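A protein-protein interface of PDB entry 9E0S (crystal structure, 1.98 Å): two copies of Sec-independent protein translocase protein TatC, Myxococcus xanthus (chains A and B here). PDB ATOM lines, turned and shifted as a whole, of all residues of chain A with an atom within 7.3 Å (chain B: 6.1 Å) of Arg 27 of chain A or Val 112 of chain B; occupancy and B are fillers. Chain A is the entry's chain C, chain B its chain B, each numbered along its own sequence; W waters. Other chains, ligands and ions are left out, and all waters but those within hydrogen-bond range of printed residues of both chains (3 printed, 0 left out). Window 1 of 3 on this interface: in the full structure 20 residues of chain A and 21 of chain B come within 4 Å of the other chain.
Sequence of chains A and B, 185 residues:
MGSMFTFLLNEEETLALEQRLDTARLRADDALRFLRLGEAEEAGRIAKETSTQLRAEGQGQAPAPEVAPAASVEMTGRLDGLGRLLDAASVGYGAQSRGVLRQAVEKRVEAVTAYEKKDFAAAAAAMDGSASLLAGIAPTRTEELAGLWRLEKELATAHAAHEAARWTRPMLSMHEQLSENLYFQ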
ATOM      1  N   ARG A  20      20.133  27.571 -10.197  1.00  0.00           N
ATOM      2  CA  ARG A  20      19.114  26.870  -9.424  1.00  0.00           C
ATOM      3  C   ARG A  20      17.812  27.663  -9.390  1.00  0.00           C
ATOM      4  O   ARG A  20      16.726  27.085  -9.521  1.00  0.00           O
ATOM      5  CB  ARG A  20      19.625  26.592  -8.008  1.00  0.00           C
ATOM      6  CG  ARG A  20      18.533  26.423  -6.963  1.00  0.00           C
ATOM      7  CD  ARG A  20      18.977  25.547  -5.792  1.00  0.00           C
ATOM      8  NE  ARG A  20      20.138  26.076  -5.084  1.00  0.00           N
ATOM      9  CZ  ARG A  20      21.379  25.626  -5.231  1.00  0.00           C
ATOM     10  NH1 ARG A  20      21.664  24.644  -6.074  1.00  0.00           N
ATOM     11  NH2 ARG A  20      22.357  26.174  -4.511  1.00  0.00           N
ATOM     12  N   LEU A  21      17.900  28.986  -9.231  1.00  0.00           N
ATOM     13  CA  LEU A  21      16.691  29.802  -9.245  1.00  0.00           C
ATOM     14  C   LEU A  21      16.071  29.847 -10.640  1.00  0.00           C
ATOM     15  O   LEU A  21      14.845  29.780 -10.784  1.00  0.00           O
ATOM     16  CB  LEU A  21      16.993  31.217  -8.742  1.00  0.00           C
ATOM     17  CG  LEU A  21      16.307  31.596  -7.420  1.00  0.00           C
ATOM     18  CD1 LEU A  21      16.749  30.674  -6.286  1.00  0.00           C
ATOM     19  CD2 LEU A  21      16.550  33.059  -7.046  1.00  0.00           C
ATOM     20  N   ASP A  22      16.894  29.985 -11.681  1.00  0.00           N
ATOM     21  CA  ASP A  22      16.347  30.013 -13.028  1.00  0.00           C
ATOM     22  C   ASP A  22      15.681  28.681 -13.364  1.00  0.00           C
ATOM     23  O   ASP A  22      14.637  28.643 -14.027  1.00  0.00           O
ATOM     24  CB  ASP A  22      17.451  30.346 -14.033  1.00  0.00           C
ATOM     25  CG  ASP A  22      17.985  31.771 -13.883  1.00  0.00           C
ATOM     26  OD1 ASP A  22      17.374  32.602 -13.164  1.00  0.00           O
ATOM     27  OD2 ASP A  22      19.034  32.060 -14.492  1.00  0.00           O
ATOM     28  N   THR A  23      16.250  27.578 -12.883  1.00  0.00           N
ATOM     29  CA  THR A  23      15.694  26.269 -13.215  1.00  0.00           C
ATOM     30  C   THR A  23      14.410  25.997 -12.438  1.00  0.00           C
ATOM     31  O   THR A  23      13.470  25.407 -12.980  1.00  0.00           O
ATOM     32  CB  THR A  23      16.736  25.170 -12.967  1.00  0.00           C
ATOM     33  OG1 THR A  23      17.797  25.321 -13.909  1.00  0.00           O
ATOM     34  CG2 THR A  23      16.129  23.791 -13.166  1.00  0.00           C
ATOM     35  N   ALA A  24      14.341  26.418 -11.173  1.00  0.00           N
ATOM     36  CA  ALA A  24      13.066  26.343 -10.467  1.00  0.00           C
ATOM     37  C   ALA A  24      12.001  27.194 -11.160  1.00  0.00           C
ATOM     38  O   ALA A  24      10.823  26.828 -11.171  1.00  0.00           O
ATOM     39  CB  ALA A  24      13.240  26.780  -9.000  1.00  0.00           C
ATOM     40  N   ARG A  25      12.396  28.321 -11.759  1.00  0.00           N
ATOM     41  CA  ARG A  25      11.438  29.114 -12.528  1.00  0.00           C
ATOM     42  C   ARG A  25      10.935  28.346 -13.753  1.00  0.00           C
ATOM     43  O   ARG A  25       9.735  28.378 -14.059  1.00  0.00           O
ATOM     44  CB  ARG A  25      12.066  30.457 -12.922  1.00  0.00           C
ATOM     45  CG  ARG A  25      11.153  31.425 -13.682  1.00  0.00           C
ATOM     46  CD  ARG A  25      10.012  31.950 -12.807  1.00  0.00           C
ATOM     47  NE  ARG A  25       8.794  31.183 -13.012  1.00  0.00           N
ATOM     48  CZ  ARG A  25       7.643  31.399 -12.384  1.00  0.00           C
ATOM     49  NH1 ARG A  25       7.548  32.264 -11.389  1.00  0.00           N
ATOM     50  NH2 ARG A  25       6.556  30.734 -12.774  1.00  0.00           N
ATOM     51  N   LEU A  26      11.836  27.650 -14.471  1.00  0.00           N
ATOM     52  CA  LEU A  26      11.407  26.837 -15.618  1.00  0.00           C
ATOM     53  C   LEU A  26      10.450  25.735 -15.179  1.00  0.00           C
ATOM     54  O   LEU A  26       9.462  25.452 -15.866  1.00  0.00           O
ATOM     55  CB  LEU A  26      12.619  26.214 -16.323  1.00  0.00           C
ATOM     56  CG  LEU A  26      13.647  27.104 -17.034  1.00  0.00           C
ATOM     57  CD1 LEU A  26      14.849  26.284 -17.490  1.00  0.00           C
ATOM     58  CD2 LEU A  26      13.027  27.808 -18.207  1.00  0.00           C
ATOM     59  N   ARG A  27      10.751  25.085 -14.046  1.00  0.00           N
ATOM     60  CA  ARG A  27       9.858  24.077 -13.472  1.00  0.00           C
ATOM     61  C   ARG A  27       8.472  24.647 -13.198  1.00  0.00           C
ATOM     62  O   ARG A  27       7.457  24.029 -13.534  1.00  0.00           O
ATOM     63  CB  ARG A  27      10.442  23.531 -12.167  1.00  0.00           C
ATOM     64  CG  ARG A  27      11.751  22.785 -12.297  1.00  0.00           C
ATOM     65  CD  ARG A  27      11.575  21.590 -13.182  1.00  0.00           C
ATOM     66  NE  ARG A  27      12.672  20.638 -13.057  1.00  0.00           N
ATOM     67  CZ  ARG A  27      12.850  19.616 -13.882  1.00  0.00           C
ATOM     68  NH1 ARG A  27      12.049  19.422 -14.923  1.00  0.00           N
ATOM     69  NH2 ARG A  27      13.857  18.771 -13.663  1.00  0.00           N
ATOM     70  N   ALA A  28       8.408  25.806 -12.537  1.00  0.00           N
ATOM     71  CA  ALA A  28       7.105  26.384 -12.230  1.00  0.00           C
ATOM     72  C   ALA A  28       6.371  26.773 -13.504  1.00  0.00           C
ATOM     73  O   ALA A  28       5.149  26.632 -13.588  1.00  0.00           O
ATOM     74  CB  ALA A  28       7.260  27.597 -11.304  1.00  0.00           C
ATOM     75  N   ASP A  29       7.101  27.269 -14.507  1.00  0.00           N
ATOM     76  CA  ASP A  29       6.470  27.570 -15.786  1.00  0.00           C
ATOM     77  C   ASP A  29       5.852  26.320 -16.399  1.00  0.00           C
ATOM     78  O   ASP A  29       4.738  26.366 -16.939  1.00  0.00           O
ATOM     79  CB  ASP A  29       7.484  28.163 -16.747  1.00  0.00           C
ATOM     80  CG  ASP A  29       7.934  29.545 -16.337  1.00  0.00           C
ATOM     81  OD1 ASP A  29       7.337  30.134 -15.402  1.00  0.00           O
ATOM     82  OD2 ASP A  29       8.908  30.019 -16.946  1.00  0.00           O
ATOM     83  N   ASP A  30       6.550  25.188 -16.318  1.00  0.00           N
ATOM     84  CA  ASP A  30       5.995  23.986 -16.928  1.00  0.00           C
ATOM     85  C   ASP A  30       4.818  23.430 -16.135  1.00  0.00           C
ATOM     86  O   ASP A  30       3.885  22.862 -16.733  1.00  0.00           O
ATOM     87  CB  ASP A  30       7.090  22.942 -17.112  1.00  0.00           C
ATOM     88  CG  ASP A  30       8.007  23.294 -18.259  1.00  0.00           C
ATOM     89  OD1 ASP A  30       7.570  24.064 -19.147  1.00  0.00           O
ATOM     90  OD2 ASP A  30       9.161  22.835 -18.265  1.00  0.00           O
ATOM     91  N   ALA A  31       4.834  23.572 -14.804  1.00  0.00           N
ATOM     92  CA  ALA A  31       3.634  23.254 -14.035  1.00  0.00           C
ATOM     93  C   ALA A  31       2.461  24.122 -14.482  1.00  0.00           C
ATOM     94  O   ALA A  31       1.338  23.632 -14.642  1.00  0.00           O
ATOM     95  CB  ALA A  31       3.898  23.438 -12.535  1.00  0.00           C
ATOM     96  N   LEU A  32       2.703  25.419 -14.703  1.00  0.00           N
ATOM     97  CA  LEU A  32       1.618  26.270 -15.185  1.00  0.00           C
ATOM     98  C   LEU A  32       1.170  25.865 -16.585  1.00  0.00           C
ATOM     99  O   LEU A  32      -0.012  26.016 -16.914  1.00  0.00           O
ATOM    100  CB  LEU A  32       2.043  27.737 -15.152  1.00  0.00           C
ATOM    101  CG  LEU A  32       2.368  28.232 -13.741  1.00  0.00           C
ATOM    102  CD1 LEU A  32       2.853  29.658 -13.778  1.00  0.00           C
ATOM    103  CD2 LEU A  32       1.127  28.115 -12.828  1.00  0.00           C
ATOM    104  N   ARG A  33       2.090  25.351 -17.418  1.00  0.00           N
ATOM    105  CA  ARG A  33       1.708  24.867 -18.742  1.00  0.00           C
ATOM    106  C   ARG A  33       0.770  23.667 -18.653  1.00  0.00           C
ATOM    107  O   ARG A  33      -0.134  23.528 -19.483  1.00  0.00           O
ATOM    108  CB  ARG A  33       2.943  24.511 -19.569  1.00  0.00           C
ATOM    109  CG  ARG A  33       3.662  25.737 -20.089  1.00  0.00           C
ATOM    110  CD  ARG A  33       4.821  25.410 -21.029  1.00  0.00           C
ATOM    111  NE  ARG A  33       5.359  26.664 -21.541  1.00  0.00           N
ATOM    112  CZ  ARG A  33       6.396  27.318 -21.036  1.00  0.00           C
ATOM    113  NH1 ARG A  33       7.172  26.783 -20.105  1.00  0.00           N
ATOM    114  NH2 ARG A  33       6.666  28.542 -21.485  1.00  0.00           N
ATOM    115  N   PHE A  34       0.962  22.790 -17.651  1.00  0.00           N
ATOM    116  CA  PHE A  34      -0.015  21.721 -17.434  1.00  0.00           C
ATOM    117  C   PHE A  34      -1.346  22.292 -16.961  1.00  0.00           C
ATOM    118  O   PHE A  34      -2.412  21.815 -17.370  1.00  0.00           O
ATOM    119  CB  PHE A  34       0.513  20.680 -16.433  1.00  0.00           C
ATOM    120  CG  PHE A  34       1.481  19.688 -17.044  1.00  0.00           C
ATOM    121  CD1 PHE A  34       1.060  18.808 -18.025  1.00  0.00           C
ATOM    122  CD2 PHE A  34       2.810  19.655 -16.643  1.00  0.00           C
ATOM    123  CE1 PHE A  34       1.947  17.901 -18.600  1.00  0.00           C
ATOM    124  CE2 PHE A  34       3.705  18.756 -17.208  1.00  0.00           C
ATOM    125  CZ  PHE A  34       3.270  17.873 -18.190  1.00  0.00           C
ATOM    126  N   ALA A  43       0.256  19.476 -12.549  1.00  0.00           N
ATOM    127  CA  ALA A  43       0.745  20.808 -12.191  1.00  0.00           C
ATOM    128  C   ALA A  43       1.084  20.885 -10.704  1.00  0.00           C
ATOM    129  O   ALA A  43       2.150  21.385 -10.320  1.00  0.00           O
ATOM    130  CB  ALA A  43      -0.296  21.871 -12.560  1.00  0.00           C
ATOM    131  N   ILE A  46       4.231  18.703  -9.682  1.00  0.00           N
ATOM    132  CA  ILE A  46       5.482  19.378 -10.022  1.00  0.00           C
ATOM    133  C   ILE A  46       5.753  20.524  -9.058  1.00  0.00           C
ATOM    134  O   ILE A  46       6.888  20.720  -8.600  1.00  0.00           O
ATOM    135  CB  ILE A  46       5.437  19.873 -11.479  1.00  0.00           C
ATOM    136  CG1 ILE A  46       5.405  18.684 -12.443  1.00  0.00           C
ATOM    137  CG2 ILE A  46       6.608  20.818 -11.757  1.00  0.00           C
ATOM    138  CD1 ILE A  46       5.272  19.083 -13.911  1.00  0.00           C
ATOM    139  N   ALA A  47       4.717  21.300  -8.736  1.00  0.00           N
ATOM    140  CA  ALA A  47       4.908  22.445  -7.853  1.00  0.00           C
ATOM    141  C   ALA A  47       5.417  22.006  -6.484  1.00  0.00           C
ATOM    142  O   ALA A  47       6.274  22.672  -5.888  1.00  0.00           O
ATOM    143  CB  ALA A  47       3.603  23.231  -7.718  1.00  0.00           C
ATOM    144  N   GLU A  49       7.112  19.137  -5.689  1.00  0.00           N
ATOM    145  CA  GLU A  49       8.498  18.698  -5.814  1.00  0.00           C
ATOM    146  C   GLU A  49       9.438  19.886  -5.948  1.00  0.00           C
ATOM    147  O   GLU A  49      10.523  19.902  -5.357  1.00  0.00           O
ATOM    148  CB  GLU A  49       8.659  17.772  -7.011  1.00  0.00           C
ATOM    149  CG  GLU A  49       8.139  16.385  -6.777  1.00  0.00           C
ATOM    150  CD  GLU A  49       8.344  15.482  -7.981  1.00  0.00           C
ATOM    151  OE1 GLU A  49       9.135  15.851  -8.888  1.00  0.00           O
ATOM    152  OE2 GLU A  49       7.701  14.408  -8.020  1.00  0.00           O
ATOM    153  N   THR A  50       9.034  20.899  -6.707  1.00  0.00           N
ATOM    154  CA  THR A  50       9.912  22.047  -6.897  1.00  0.00           C
ATOM    155  C   THR A  50      10.094  22.814  -5.592  1.00  0.00           C
ATOM    156  O   THR A  50      11.220  23.170  -5.228  1.00  0.00           O
ATOM    157  CB  THR A  50       9.353  22.957  -7.992  1.00  0.00           C
ATOM    158  OG1 THR A  50       9.146  22.187  -9.185  1.00  0.00           O
ATOM    159  CG2 THR A  50      10.326  24.087  -8.288  1.00  0.00           C
ATOM    160  N   GLN A  53      12.403  20.797  -3.183  1.00  0.00           N
ATOM    161  CA  GLN A  53      13.813  20.858  -3.547  1.00  0.00           C
ATOM    162  C   GLN A  53      14.374  22.258  -3.336  1.00  0.00           C
ATOM    163  O   GLN A  53      15.498  22.416  -2.846  1.00  0.00           O
ATOM    164  CB  GLN A  53      14.015  20.420  -4.998  1.00  0.00           C
ATOM    165  CG  GLN A  53      15.450  20.607  -5.478  1.00  0.00           C
ATOM    166  CD  GLN A  53      15.674  20.123  -6.900  1.00  0.00           C
ATOM    167  OE1 GLN A  53      15.073  19.141  -7.341  1.00  0.00           O
ATOM    168  NE2 GLN A  53      16.549  20.812  -7.626  1.00  0.00           N
ATOM    169  N   LEU A 148       0.676  25.414  -6.174  1.00  0.00           N
ATOM    170  CA  LEU A 148       1.170  26.312  -7.212  1.00  0.00           C
ATOM    171  C   LEU A 148       1.370  27.724  -6.680  1.00  0.00           C
ATOM    172  O   LEU A 148       2.365  28.378  -7.010  1.00  0.00           O
ATOM    173  CB  LEU A 148       0.199  26.328  -8.393  1.00  0.00           C
ATOM    174  CG  LEU A 148       0.244  25.064  -9.242  1.00  0.00           C
ATOM    175  CD1 LEU A 148      -1.039  24.926 -10.050  1.00  0.00           C
ATOM    176  CD2 LEU A 148       1.471  25.116 -10.149  1.00  0.00           C
ATOM    177  N   LEU A 151       4.429  27.997  -4.458  1.00  0.00           N
ATOM    178  CA  LEU A 151       5.651  28.018  -5.256  1.00  0.00           C
ATOM    179  C   LEU A 151       5.887  29.399  -5.861  1.00  0.00           C
ATOM    180  O   LEU A 151       7.021  29.891  -5.874  1.00  0.00           O
ATOM    181  CB  LEU A 151       5.593  26.949  -6.349  1.00  0.00           C
ATOM    182  CG  LEU A 151       6.807  26.877  -7.277  1.00  0.00           C
ATOM    183  CD1 LEU A 151       8.078  26.696  -6.448  1.00  0.00           C
ATOM    184  CD2 LEU A 151       6.640  25.733  -8.250  1.00  0.00           C
ATOM    185  N   LEU A 155       9.154  31.522  -5.055  1.00  0.00           N
ATOM    186  CA  LEU A 155      10.054  31.973  -6.110  1.00  0.00           C
ATOM    187  C   LEU A 155      10.216  33.488  -6.093  1.00  0.00           C
ATOM    188  O   LEU A 155      11.321  33.998  -6.313  1.00  0.00           O
ATOM    189  CB  LEU A 155       9.543  31.502  -7.479  1.00  0.00           C
ATOM    190  CG  LEU A 155       9.741  30.028  -7.817  1.00  0.00           C
ATOM    191  CD1 LEU A 155       9.086  29.692  -9.152  1.00  0.00           C
ATOM    192  CD2 LEU A 155      11.222  29.688  -7.847  1.00  0.00           C
ATOM    193  N   LEU B  79      15.174  26.570 -24.883  1.00  0.00           N
ATOM    194  CA  LEU B  79      14.069  26.276 -23.974  1.00  0.00           C
ATOM    195  C   LEU B  79      13.009  27.368 -24.026  1.00  0.00           C
ATOM    196  O   LEU B  79      11.811  27.079 -24.010  1.00  0.00           O
ATOM    197  CB  LEU B  79      14.583  26.114 -22.540  1.00  0.00           C
ATOM    198  CG  LEU B  79      15.233  24.760 -22.246  1.00  0.00           C
ATOM    199  CD1 LEU B  79      15.891  24.783 -20.879  1.00  0.00           C
ATOM    200  CD2 LEU B  79      14.192  23.626 -22.336  1.00  0.00           C
ATOM    201  N   LYS B 107       7.444  16.291 -22.729  1.00  0.00           N
ATOM    202  CA  LYS B 107       8.781  16.242 -23.324  1.00  0.00           C
ATOM    203  C   LYS B 107       9.606  17.469 -22.943  1.00  0.00           C
ATOM    204  O   LYS B 107      10.820  17.376 -22.718  1.00  0.00           O
ATOM    205  CB  LYS B 107       8.678  16.115 -24.843  1.00  0.00           C
ATOM    206  CG  LYS B 107       8.446  14.703 -25.282  1.00  0.00           C
ATOM    207  CD  LYS B 107       9.777  13.975 -25.295  1.00  0.00           C
ATOM    208  CE  LYS B 107       9.677  12.709 -24.524  1.00  0.00           C
ATOM    209  NZ  LYS B 107      10.964  11.975 -24.587  1.00  0.00           N
ATOM    210  N   ARG B 108       8.976  18.633 -22.892  1.00  0.00           N
ATOM    211  CA  ARG B 108       9.705  19.823 -22.476  1.00  0.00           C
ATOM    212  C   ARG B 108      10.159  19.711 -21.020  1.00  0.00           C
ATOM    213  O   ARG B 108      11.239  20.197 -20.664  1.00  0.00           O
ATOM    214  CB  ARG B 108       8.820  21.047 -22.723  1.00  0.00           C
ATOM    215  CG  ARG B 108       8.851  22.091 -21.648  1.00  0.00           C
ATOM    216  CD  ARG B 108       9.890  23.161 -21.868  1.00  0.00           C
ATOM    217  NE  ARG B 108       9.988  23.926 -20.627  1.00  0.00           N
ATOM    218  CZ  ARG B 108      10.354  25.196 -20.518  1.00  0.00           C
ATOM    219  NH1 ARG B 108      10.745  25.902 -21.570  1.00  0.00           N
ATOM    220  NH2 ARG B 108      10.318  25.774 -19.317  1.00  0.00           N
ATOM    221  N   VAL B 109       9.369  19.047 -20.173  1.00  0.00           N
ATOM    222  CA  VAL B 109       9.807  18.800 -18.799  1.00  0.00           C
ATOM    223  C   VAL B 109      11.057  17.915 -18.783  1.00  0.00           C
ATOM    224  O   VAL B 109      12.003  18.162 -18.023  1.00  0.00           O
ATOM    225  CB  VAL B 109       8.655  18.185 -17.976  1.00  0.00           C
ATOM    226  CG1 VAL B 109       9.136  17.779 -16.600  1.00  0.00           C
ATOM    227  CG2 VAL B 109       7.496  19.180 -17.838  1.00  0.00           C
ATOM    228  N   GLU B 110      11.083  16.868 -19.614  1.00  0.00           N
ATOM    229  CA  GLU B 110      12.304  16.070 -19.742  1.00  0.00           C
ATOM    230  C   GLU B 110      13.478  16.900 -20.259  1.00  0.00           C
ATOM    231  O   GLU B 110      14.638  16.635 -19.904  1.00  0.00           O
ATOM    232  CB  GLU B 110      12.070  14.870 -20.668  1.00  0.00           C
ATOM    233  CG  GLU B 110      11.036  13.882 -20.155  1.00  0.00           C
ATOM    234  CD  GLU B 110      10.745  12.768 -21.162  1.00  0.00           C
ATOM    235  OE1 GLU B 110      11.620  12.498 -22.021  1.00  0.00           O
ATOM    236  OE2 GLU B 110       9.641  12.175 -21.098  1.00  0.00           O
ATOM    237  N   ALA B 111      13.217  17.887 -21.119  1.00  0.00           N
ATOM    238  CA  ALA B 111      14.317  18.725 -21.586  1.00  0.00           C
ATOM    239  C   ALA B 111      14.915  19.521 -20.435  1.00  0.00           C
ATOM    240  O   ALA B 111      16.140  19.650 -20.333  1.00  0.00           O
ATOM    241  CB  ALA B 111      13.854  19.670 -22.692  1.00  0.00           C
ATOM    242  N   VAL B 112      14.065  20.045 -19.549  1.00  0.00           N
ATOM    243  CA  VAL B 112      14.568  20.834 -18.421  1.00  0.00           C
ATOM    244  C   VAL B 112      15.338  19.939 -17.453  1.00  0.00           C
ATOM    245  O   VAL B 112      16.372  20.338 -16.908  1.00  0.00           O
ATOM    246  CB  VAL B 112      13.417  21.577 -17.719  1.00  0.00           C
ATOM    247  CG1 VAL B 112      13.913  22.277 -16.424  1.00  0.00           C
ATOM    248  CG2 VAL B 112      12.753  22.593 -18.691  1.00  0.00           C
ATOM    249  N   THR B 113      14.856  18.715 -17.238  1.00  0.00           N
ATOM    250  CA  THR B 113      15.584  17.754 -16.411  1.00  0.00           C
ATOM    251  C   THR B 113      16.972  17.461 -16.983  1.00  0.00           C
ATOM    252  O   THR B 113      17.966  17.439 -16.250  1.00  0.00           O
ATOM    253  CB  THR B 113      14.773  16.462 -16.283  1.00  0.00           C
ATOM    254  OG1 THR B 113      13.568  16.716 -15.551  1.00  0.00           O
ATOM    255  CG2 THR B 113      15.584  15.394 -15.569  1.00  0.00           C
ATOM    256  N   ALA B 114      17.055  17.221 -18.296  1.00  0.00           N
ATOM    257  CA  ALA B 114      18.351  16.998 -18.936  1.00  0.00           C
ATOM    258  C   ALA B 114      19.235  18.225 -18.806  1.00  0.00           C
ATOM    259  O   ALA B 114      20.430  18.117 -18.506  1.00  0.00           O
ATOM    260  CB  ALA B 114      18.170  16.644 -20.416  1.00  0.00           C
ATOM    261  N   TYR B 115      18.655  19.403 -19.036  1.00  0.00           N
ATOM    262  CA  TYR B 115      19.371  20.662 -18.903  1.00  0.00           C
ATOM    263  C   TYR B 115      19.935  20.834 -17.496  1.00  0.00           C
ATOM    264  O   TYR B 115      21.079  21.268 -17.331  1.00  0.00           O
ATOM    265  CB  TYR B 115      18.421  21.800 -19.263  1.00  0.00           C
ATOM    266  CG  TYR B 115      18.923  23.192 -19.015  1.00  0.00           C
ATOM    267  CD1 TYR B 115      19.781  23.814 -19.919  1.00  0.00           C
ATOM    268  CD2 TYR B 115      18.490  23.911 -17.910  1.00  0.00           C
ATOM    269  CE1 TYR B 115      20.214  25.111 -19.710  1.00  0.00           C
ATOM    270  CE2 TYR B 115      18.913  25.209 -17.696  1.00  0.00           C
ATOM    271  CZ  TYR B 115      19.775  25.799 -18.594  1.00  0.00           C
ATOM    272  OH  TYR B 115      20.201  27.083 -18.380  1.00  0.00           O
ATOM    273  N   GLU B 116      19.151  20.469 -16.475  1.00  0.00           N
ATOM    274  CA  GLU B 116      19.591  20.577 -15.084  1.00  0.00           C
ATOM    275  C   GLU B 116      20.769  19.654 -14.776  1.00  0.00           C
ATOM    276  O   GLU B 116      21.617  19.987 -13.938  1.00  0.00           O
ATOM    277  CB  GLU B 116      18.424  20.266 -14.148  1.00  0.00           C
ATOM    278  CG  GLU B 116      18.758  20.372 -12.669  1.00  0.00           C
ATOM    279  CD  GLU B 116      17.582  19.987 -11.793  1.00  0.00           C
ATOM    280  OE1 GLU B 116      16.939  18.963 -12.094  1.00  0.00           O
ATOM    281  OE2 GLU B 116      17.280  20.725 -10.825  1.00  0.00           O
ATOM    282  N   LYS B 117      20.831  18.492 -15.423  1.00  0.00           N
ATOM    283  CA  LYS B 117      21.960  17.582 -15.286  1.00  0.00           C
ATOM    284  C   LYS B 117      23.133  17.978 -16.165  1.00  0.00           C
ATOM    285  O   LYS B 117      24.130  17.256 -16.193  1.00  0.00           O
ATOM    286  CB  LYS B 117      21.550  16.148 -15.652  1.00  0.00           C
ATOM    287  CG  LYS B 117      20.342  15.601 -14.937  1.00  0.00           C
ATOM    288  CD  LYS B 117      19.949  14.248 -15.528  1.00  0.00           C
ATOM    289  CE  LYS B 117      18.672  13.696 -14.896  1.00  0.00           C
ATOM    290  NZ  LYS B 117      18.035  12.608 -15.727  1.00  0.00           N
ATOM    291  N   ALA B 123      18.949  17.292 -23.697  1.00  0.00           N
ATOM    292  CA  ALA B 123      18.028  18.426 -23.687  1.00  0.00           C
ATOM    293  C   ALA B 123      17.572  18.762 -25.100  1.00  0.00           C
ATOM    294  O   ALA B 123      16.373  18.864 -25.364  1.00  0.00           O
ATOM    295  CB  ALA B 123      18.692  19.642 -23.026  1.00  0.00           C
HETATM  296  O   HOH W   1      14.367  20.746 -10.683  1.00  0.00           O
HETATM  297  O   HOH W   2       9.524  28.581 -19.306  1.00  0.00           O
HETATM  298  O   HOH W   3      19.798  27.390 -15.026  1.00  0.00           O
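O of Leu 79 of chain B sits at hydrogen-bond distance from NH1 of Arg 108 of chain B (2.9 Å).
The side-chain hydroxyl of Thr 113 of chain B sits at hydrogen-bond distance from the backbone carbonyl oxygen of Val 109 of chain B, 3.3 Å away.
OD1 of Asp 30 of chain A is in salt-bridge range of NH1 of Arg 33 of chain A (2.9 Å).
Among the printed residues, merely in contact across the chains: Thr 23 of chain A with Tyr 115 of chain B (3.9 Å), Leu 26 of chain A with Leu 79 of chain B (3.9 Å), Leu 26 of chain A with Arg 108 of chain B (3.6 Å), Arg 27 of chain A with Val 112 of chain B (3.7 Å), Asp 30 of chain A with Val 109 of chain B (3.9 Å), Asp 30 of chain A with Val 112 of chain B (3.6 Å) and Phe 34 of chain A with Val 109 of chain B (3.9 Å).
Printed residues of chain B that touch a printed residue of chain A: Leu 79, Arg 108, Val 109, Val 112, Thr 113, Tyr 115 and Glu 116.
Among the printed residues, Asp or Glu carboxylates within 4 Å of a Lys or Arg side-chain nitrogen of the other chain: Arg 27 of chain A with Glu 116 of chain B and Asp 30 of chain A with Arg 108 of chain B.
The side-chain hydroxyl (OG1) of Thr 113 of chain B lies within hydrogen-bond range of the guanidinium group (NH2) of Arg 27 of chain A.
O of Val 109 of chain B is in hydrogen-bond range of NH1 of Arg 27 of chain A (3.3 Å).
The side-chain carboxylate (OE1) of Glu 116 of chain B lies within salt-bridge range of the guanidinium group (NH2) of Arg 27 of chain A.
The guanidinium group of Arg 33 of chain A lies close to the guanidinium group of Arg 108 of chain B (3.4 Å).
The side-chain carboxylate (OD2) of Asp 30 of chain A lies within salt-bridge range of the guanidinium group (NE) of Arg 108 of chain B (2.7 Å).
The side-chain amide nitrogen (NE2) of Gln 53 of chain A lies within hydrogen-bond range of the side-chain carboxylate (OE2) of Glu 116 of chain B, 3.3 Å away.
Water W2 lies within hydrogen-bond range of the side-chain carboxylate (OD2) of Asp 29 of chain A (2.8 Å), the guanidinium group (NH2) of Arg 108 of chain B (2.9 Å) and the guanidinium group (NH1) of Arg 33 of chain A (3.1 Å).
Water W1 lies within hydrogen-bond range of OE2 of Glu 116 of chain B and NE of Arg 27 of chain A.
Water W3 lies within hydrogen-bond range of OG1 of Thr 23 of chain A (3.1 Å) and OH of Tyr 115 of chain B (3.4 Å).
Of the printed residues of chain B, Arg 27 of chain A touches Val 109 (3.3 Å), Val 112 (3.7 Å), Thr 113 (2.8 Å) and Glu 116 (3.5 Å).
Val 112 of chain B touches just these residues of chain A: Arg 27 and Asp 30.
No residue of chain A comes within 4 Å of Ala 111 of chain B.
Of the printed residues of chain B, Leu 26 of chain A touches Leu 79 (3.9 Å) and Arg 108 (3.6 Å).
Of the printed residues of chain B, Arg 33 of chain A touches Arg 108.
Printed residues of chain A within 4 Å of Val 109 of chain B: Arg 27 (3.3 Å), Asp 30 (3.9 Å) and Phe 34 (3.9 Å).
Printed residues of chain B within 4 Å of Phe 34 of chain A: Val 109.
Of the printed residues of chain A, Leu 79 of chain B touches Leu 26.
Arg 25 of chain A touches none of the printed residues of chain B.
The nearest printed residue of chain B that does not touch Phe 34 of chain A is Lys 107 of chain B (6.4 Å).
No position is printed for both chains.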
